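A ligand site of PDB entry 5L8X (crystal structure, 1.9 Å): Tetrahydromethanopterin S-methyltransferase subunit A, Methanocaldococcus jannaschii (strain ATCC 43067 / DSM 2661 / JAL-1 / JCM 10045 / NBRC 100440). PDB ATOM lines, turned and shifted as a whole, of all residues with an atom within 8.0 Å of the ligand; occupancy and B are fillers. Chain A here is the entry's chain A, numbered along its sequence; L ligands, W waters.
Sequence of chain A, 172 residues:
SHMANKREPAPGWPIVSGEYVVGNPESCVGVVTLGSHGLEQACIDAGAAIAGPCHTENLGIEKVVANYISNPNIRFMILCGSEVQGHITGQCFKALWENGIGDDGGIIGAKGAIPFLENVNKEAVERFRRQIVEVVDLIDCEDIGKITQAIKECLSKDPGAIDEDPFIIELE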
ATOM      1  N   VAL A  16      23.230 -21.182  13.525  1.00  0.00           N
ATOM      2  CA  VAL A  16      22.515 -22.091  12.626  1.00  0.00           C
ATOM      3  C   VAL A  16      21.361 -21.378  11.927  1.00  0.00           C
ATOM      4  O   VAL A  16      20.479 -20.829  12.584  1.00  0.00           O
ATOM      5  CB  VAL A  16      21.984 -23.311  13.396  1.00  0.00           C
ATOM      6  CG1 VAL A  16      21.080 -24.170  12.518  1.00  0.00           C
ATOM      7  CG2 VAL A  16      23.161 -24.134  13.941  1.00  0.00           C
ATOM      8  N   SER A  17      21.378 -21.367  10.594  1.00  0.00           N
ATOM      9  CA  SER A  17      20.326 -20.712   9.820  1.00  0.00           C
ATOM     10  C   SER A  17      19.001 -21.487   9.951  1.00  0.00           C
ATOM     11  O   SER A  17      18.993 -22.715  10.061  1.00  0.00           O
ATOM     12  CB  SER A  17      20.704 -20.601   8.345  1.00  0.00           C
ATOM     13  OG  SER A  17      21.874 -19.797   8.207  1.00  0.00           O
ATOM     14  N   GLY A  18      17.883 -20.773   9.936  1.00  0.00           N
ATOM     15  CA  GLY A  18      16.611 -21.464   9.965  1.00  0.00           C
ATOM     16  C   GLY A  18      15.439 -20.527   9.916  1.00  0.00           C
ATOM     17  O   GLY A  18      15.573 -19.383   9.490  1.00  0.00           O
ATOM     18  N   GLU A  19      14.268 -21.039  10.282  1.00  0.00           N
ATOM     19  CA  GLU A  19      13.036 -20.250  10.297  1.00  0.00           C
ATOM     20  C   GLU A  19      12.771 -19.725  11.695  1.00  0.00           C
ATOM     21  O   GLU A  19      12.239 -20.446  12.552  1.00  0.00           O
ATOM     22  CB  GLU A  19      11.850 -21.074   9.799  1.00  0.00           C
ATOM     23  CG  GLU A  19      11.977 -21.567   8.354  1.00  0.00           C
ATOM     24  CD  GLU A  19      12.116 -20.421   7.359  1.00  0.00           C
ATOM     25  OE1 GLU A  19      11.427 -19.390   7.539  1.00  0.00           O
ATOM     26  OE2 GLU A  19      12.905 -20.549   6.404  1.00  0.00           O
ATOM     27  N   TYR A  20      13.171 -18.488  11.950  1.00  0.00           N
ATOM     28  CA  TYR A  20      12.948 -17.863  13.255  1.00  0.00           C
ATOM     29  C   TYR A  20      13.119 -16.378  13.118  1.00  0.00           C
ATOM     30  O   TYR A  20      13.654 -15.916  12.112  1.00  0.00           O
ATOM     31  CB  TYR A  20      13.923 -18.406  14.319  1.00  0.00           C
ATOM     32  CG  TYR A  20      15.388 -18.400  13.884  1.00  0.00           C
ATOM     33  CD1 TYR A  20      16.148 -17.222  13.892  1.00  0.00           C
ATOM     34  CD2 TYR A  20      16.002 -19.573  13.489  1.00  0.00           C
ATOM     35  CE1 TYR A  20      17.481 -17.224  13.503  1.00  0.00           C
ATOM     36  CE2 TYR A  20      17.322 -19.574  13.082  1.00  0.00           C
ATOM     37  CZ  TYR A  20      18.057 -18.417  13.090  1.00  0.00           C
ATOM     38  OH  TYR A  20      19.379 -18.471  12.675  1.00  0.00           O
ATOM     39  N   LEU A  34       6.071 -24.563  17.072  1.00  0.00           N
ATOM     40  CA  LEU A  34       5.640 -25.820  16.449  1.00  0.00           C
ATOM     41  C   LEU A  34       4.971 -25.597  15.087  1.00  0.00           C
ATOM     42  O   LEU A  34       5.591 -25.012  14.208  1.00  0.00           O
ATOM     43  CB  LEU A  34       4.699 -26.596  17.399  1.00  0.00           C
ATOM     44  CG  LEU A  34       5.345 -26.872  18.789  1.00  0.00           C
ATOM     45  CD1 LEU A  34       4.387 -27.548  19.767  1.00  0.00           C
ATOM     46  CD2 LEU A  34       6.614 -27.693  18.661  1.00  0.00           C
ATOM     47  N   GLY A  52      10.402 -19.163  16.881  1.00  0.00           N
ATOM     48  CA  GLY A  52      10.226 -19.761  15.569  1.00  0.00           C
ATOM     49  C   GLY A  52       9.535 -21.097  15.622  1.00  0.00           C
ATOM     50  O   GLY A  52       9.428 -21.706  16.691  1.00  0.00           O
ATOM     51  N   PRO A  53       9.045 -21.559  14.459  1.00  0.00           N
ATOM     52  CA  PRO A  53       8.380 -22.863  14.312  1.00  0.00           C
ATOM     53  C   PRO A  53       9.364 -24.012  14.439  1.00  0.00           C
ATOM     54  O   PRO A  53      10.583 -23.827  14.373  1.00  0.00           O
ATOM     55  CB  PRO A  53       7.812 -22.822  12.877  1.00  0.00           C
ATOM     56  CG  PRO A  53       8.719 -21.864  12.152  1.00  0.00           C
ATOM     57  CD  PRO A  53       9.131 -20.832  13.172  1.00  0.00           C
ATOM     58  N   CYS A  54       8.835 -25.209  14.621  1.00  0.00           N
ATOM     59  CA  CYS A  54       9.669 -26.396  14.625  1.00  0.00           C
ATOM     60  C   CYS A  54       8.817 -27.515  14.057  1.00  0.00           C
ATOM     61  O   CYS A  54       7.900 -28.017  14.716  1.00  0.00           O
ATOM     62  CB  CYS A  54      10.176 -26.708  16.030  1.00  0.00           C
ATOM     63  SG  CYS A  54      11.372 -28.065  16.077  1.00  0.00           S
ATOM     64  N   HIS A  55       9.134 -27.916  12.832  1.00  0.00           N
ATOM     65  CA  HIS A  55       8.282 -28.862  12.096  1.00  0.00           C
ATOM     66  C   HIS A  55       8.691 -30.309  12.358  1.00  0.00           C
ATOM     67  O   HIS A  55       7.830 -31.161  12.594  1.00  0.00           O
ATOM     68  CB  HIS A  55       8.315 -28.551  10.598  1.00  0.00           C
ATOM     69  CG  HIS A  55       8.058 -27.119  10.262  1.00  0.00           C
ATOM     70  ND1 HIS A  55       6.817 -26.522  10.403  1.00  0.00           N
ATOM     71  CD2 HIS A  55       8.890 -26.146   9.804  1.00  0.00           C
ATOM     72  CE1 HIS A  55       6.898 -25.256  10.033  1.00  0.00           C
ATOM     73  NE2 HIS A  55       8.137 -24.998   9.676  1.00  0.00           N
ATOM     74  N   THR A  56       9.982 -30.611  12.264  1.00  0.00           N
ATOM     75  CA  THR A  56      10.395 -32.010  12.389  1.00  0.00           C
ATOM     76  C   THR A  56      10.999 -32.314  13.741  1.00  0.00           C
ATOM     77  O   THR A  56      11.566 -31.448  14.415  1.00  0.00           O
ATOM     78  CB  THR A  56      11.386 -32.416  11.278  1.00  0.00           C
ATOM     79  OG1 THR A  56      12.547 -31.576  11.350  1.00  0.00           O
ATOM     80  CG2 THR A  56      10.740 -32.234   9.890  1.00  0.00           C
ATOM     81  N   GLU A  57      10.848 -33.570  14.140  1.00  0.00           N
ATOM     82  CA  GLU A  57      11.269 -34.059  15.452  1.00  0.00           C
ATOM     83  C   GLU A  57      12.705 -34.574  15.404  1.00  0.00           C
ATOM     84  O   GLU A  57      13.166 -35.246  16.331  1.00  0.00           O
ATOM     85  CB  GLU A  57      10.303 -35.182  15.904  1.00  0.00           C
ATOM     86  CG  GLU A  57      10.433 -36.493  15.117  1.00  0.00           C
ATOM     87  CD  GLU A  57       9.709 -36.471  13.771  1.00  0.00           C
ATOM     88  OE1 GLU A  57       9.415 -35.380  13.241  1.00  0.00           O
ATOM     89  OE2 GLU A  57       9.410 -37.567  13.239  1.00  0.00           O
ATOM     90  N   ASN A  58      13.407 -34.256  14.318  1.00  0.00           N
ATOM     91  CA  ASN A  58      14.822 -34.596  14.191  1.00  0.00           C
ATOM     92  C   ASN A  58      15.618 -33.334  13.877  1.00  0.00           C
ATOM     93  O   ASN A  58      16.163 -32.683  14.790  1.00  0.00           O
ATOM     94  CB  ASN A  58      15.021 -35.701  13.129  1.00  0.00           C
ATOM     95  CG  ASN A  58      14.057 -35.580  11.967  1.00  0.00           C
ATOM     96  OD1 ASN A  58      14.128 -34.618  11.186  1.00  0.00           O
ATOM     97  ND2 ASN A  58      13.130 -36.546  11.828  1.00  0.00           N
ATOM     98  N   LEU A  59      15.676 -32.945  12.611  1.00  0.00           N
ATOM     99  CA  LEU A  59      16.396 -31.715  12.226  1.00  0.00           C
ATOM    100  C   LEU A  59      15.894 -30.472  12.951  1.00  0.00           C
ATOM    101  O   LEU A  59      16.688 -29.613  13.343  1.00  0.00           O
ATOM    102  CB  LEU A  59      16.284 -31.480  10.721  1.00  0.00           C
ATOM    103  CG  LEU A  59      16.905 -30.204  10.152  1.00  0.00           C
ATOM    104  CD1 LEU A  59      18.418 -30.146  10.331  1.00  0.00           C
ATOM    105  CD2 LEU A  59      16.496 -30.021   8.680  1.00  0.00           C
ATOM    106  N   GLY A  60      14.570 -30.347  13.085  1.00  0.00           N
ATOM    107  CA  GLY A  60      13.979 -29.171  13.713  1.00  0.00           C
ATOM    108  C   GLY A  60      14.456 -29.037  15.149  1.00  0.00           C
ATOM    109  O   GLY A  60      14.894 -27.954  15.589  1.00  0.00           O
ATOM    110  N   ILE A  61      14.375 -30.140  15.890  1.00  0.00           N
ATOM    111  CA  ILE A  61      14.837 -30.157  17.267  1.00  0.00           C
ATOM    112  C   ILE A  61      16.338 -29.825  17.337  1.00  0.00           C
ATOM    113  O   ILE A  61      16.762 -29.063  18.206  1.00  0.00           O
ATOM    114  CB  ILE A  61      14.539 -31.521  17.919  1.00  0.00           C
ATOM    115  CG1 ILE A  61      13.024 -31.710  18.018  1.00  0.00           C
ATOM    116  CG2 ILE A  61      15.249 -31.676  19.258  1.00  0.00           C
ATOM    117  CD1 ILE A  61      12.563 -32.976  18.710  1.00  0.00           C
ATOM    118  N   GLU A  62      17.150 -30.396  16.440  1.00  0.00           N
ATOM    119  CA  GLU A  62      18.571 -30.083  16.455  1.00  0.00           C
ATOM    120  C   GLU A  62      18.854 -28.599  16.275  1.00  0.00           C
ATOM    121  O   GLU A  62      19.643 -28.038  17.025  1.00  0.00           O
ATOM    122  CB  GLU A  62      19.360 -30.866  15.388  1.00  0.00           C
ATOM    123  CG  GLU A  62      19.428 -32.355  15.678  1.00  0.00           C
ATOM    124  CD  GLU A  62      20.510 -33.040  14.861  1.00  0.00           C
ATOM    125  OE1 GLU A  62      21.127 -34.000  15.401  1.00  0.00           O
ATOM    126  OE2 GLU A  62      20.768 -32.618  13.720  1.00  0.00           O
ATOM    127  N   LYS A  63      18.184 -27.951  15.321  1.00  0.00           N
ATOM    128  CA  LYS A  63      18.488 -26.533  15.097  1.00  0.00           C
ATOM    129  C   LYS A  63      18.113 -25.675  16.326  1.00  0.00           C
ATOM    130  O   LYS A  63      18.792 -24.690  16.635  1.00  0.00           O
ATOM    131  CB  LYS A  63      17.731 -26.012  13.885  1.00  0.00           C
ATOM    132  CG  LYS A  63      18.089 -26.671  12.572  1.00  0.00           C
ATOM    133  CD  LYS A  63      17.732 -25.685  11.444  1.00  0.00           C
ATOM    134  CE  LYS A  63      18.124 -26.211  10.075  1.00  0.00           C
ATOM    135  NZ  LYS A  63      17.806 -25.199   9.027  1.00  0.00           N
ATOM    136  N   VAL A  64      17.051 -26.058  17.035  1.00  0.00           N
ATOM    137  CA  VAL A  64      16.689 -25.314  18.232  1.00  0.00           C
ATOM    138  C   VAL A  64      17.713 -25.561  19.343  1.00  0.00           C
ATOM    139  O   VAL A  64      18.216 -24.614  19.944  1.00  0.00           O
ATOM    140  CB  VAL A  64      15.266 -25.674  18.746  1.00  0.00           C
ATOM    141  CG1 VAL A  64      14.985 -25.012  20.087  1.00  0.00           C
ATOM    142  CG2 VAL A  64      14.185 -25.248  17.721  1.00  0.00           C
ATOM    143  N   HIS A  87       4.566 -36.233  13.397  1.00  0.00           N
ATOM    144  CA  HIS A  87       5.812 -35.738  13.969  1.00  0.00           C
ATOM    145  C   HIS A  87       5.727 -35.600  15.493  1.00  0.00           C
ATOM    146  O   HIS A  87       6.660 -35.969  16.204  1.00  0.00           O
ATOM    147  CB  HIS A  87       6.192 -34.401  13.332  1.00  0.00           C
ATOM    148  CG  HIS A  87       6.407 -34.484  11.856  1.00  0.00           C
ATOM    149  ND1 HIS A  87       7.557 -35.014  11.311  1.00  0.00           N
ATOM    150  CD2 HIS A  87       5.635 -34.091  10.809  1.00  0.00           C
ATOM    151  CE1 HIS A  87       7.485 -34.951   9.993  1.00  0.00           C
ATOM    152  NE2 HIS A  87       6.341 -34.403   9.658  1.00  0.00           N
ATOM    153  N   THR A  89       6.047 -33.122  17.447  1.00  0.00           N
ATOM    154  CA  THR A  89       7.323 -32.491  17.743  1.00  0.00           C
ATOM    155  C   THR A  89       7.394 -31.919  19.162  1.00  0.00           C
ATOM    156  O   THR A  89       8.444 -32.001  19.821  1.00  0.00           O
ATOM    157  CB  THR A  89       7.600 -31.410  16.674  1.00  0.00           C
ATOM    158  OG1 THR A  89       7.681 -32.055  15.381  1.00  0.00           O
ATOM    159  CG2 THR A  89       8.900 -30.653  16.959  1.00  0.00           C
HETATM  160  C1  LIG L   1      14.571 -25.927   8.635  1.00  0.00           C
HETATM  161  O1  LIG L   1      14.979 -26.381   7.545  1.00  0.00           O
HETATM  162  O2  LIG L   1      15.221 -25.045   9.246  1.00  0.00           O
HETATM  163  C2  LIG L   1      13.288 -26.438   9.234  1.00  0.00           C
HETATM  164  O3  LIG L   1      12.417 -26.943   8.226  1.00  0.00           O
HETATM  165  C3  LIG L   1      13.579 -27.509  10.273  1.00  0.00           C
HETATM  166  C4  LIG L   1      12.255 -27.908  10.884  1.00  0.00           C
HETATM  167  O4  LIG L   1      11.546 -27.088  11.529  1.00  0.00           O
HETATM  168  O5  LIG L   1      11.860 -29.081  10.709  1.00  0.00           O
HETATM  169  O   HOH W   1      12.999 -29.688   7.860  1.00  0.00           O
HETATM  170  O   HOH W   2      14.350 -23.750  11.182  1.00  0.00           O
HETATM  171  O   HOH W   3      11.897 -24.621  11.850  1.00  0.00           O
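Merely in contact with the ligand: Gly 18, Cys 54 and Gly 60.
Hydrophobic or aromatic side chains within 4 Å of the ligand: His 55.
Of the 21 residues printed, 6 come within 4 Å of the ligand.
The nearest printed residue that does not touch the ligand is Leu 59 (4.1 Å).
The side-chain amino group of Lys 63 lies within salt-bridge range of an oxygen (O2) of the ligand (2.6 Å).
The backbone NH of Thr 56 lies within hydrogen-bond range of an oxygen (O5) of the ligand (2.9 Å).
OG1 of Thr 56 sits at hydrogen-bond distance from O5 of the ligand, at 2.7 Å.
N of His 55 sits at hydrogen-bond distance from O4 of the ligand (2.9 Å).
Water W2 bridges an oxygen (O2) of the ligand (2.5 Å) and the backbone NH (N) of Glu 19 (2.9 Å).
Water W3 lies within hydrogen-bond range of O4 of the ligand (2.5 Å) and O of Pro 53 (3.0 Å).
The backbone carbonyl oxygen (O) of Ser 17 is in hydrogen-bond range of the side-chain amino group (NZ) of Lys 63 (2.9 Å).
OG1 of Thr 56 is in hydrogen-bond range of N of Gly 60, at 2.9 Å.
O of Thr 56 sits at hydrogen-bond distance from SG of Cys 54, 3.8 Å away.
The side-chain amide oxygen (OD1) of Asn 58 is in hydrogen-bond range of the side-chain hydroxyl (OG1) of Thr 56, 3.4 Å away.
The side-chain hydroxyl (OG1) of Thr 89 is in hydrogen-bond range of the backbone carbonyl oxygen (O) of His 55.
O of Gly 60 lies close to SG of Cys 54 (3.6 Å).
SG of Cys 54 is in hydrogen-bond range of N of Ile 61 (3.7 Å).
The backbone NH of Cys 54 sits at hydrogen-bond distance from the backbone carbonyl oxygen of Leu 34.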
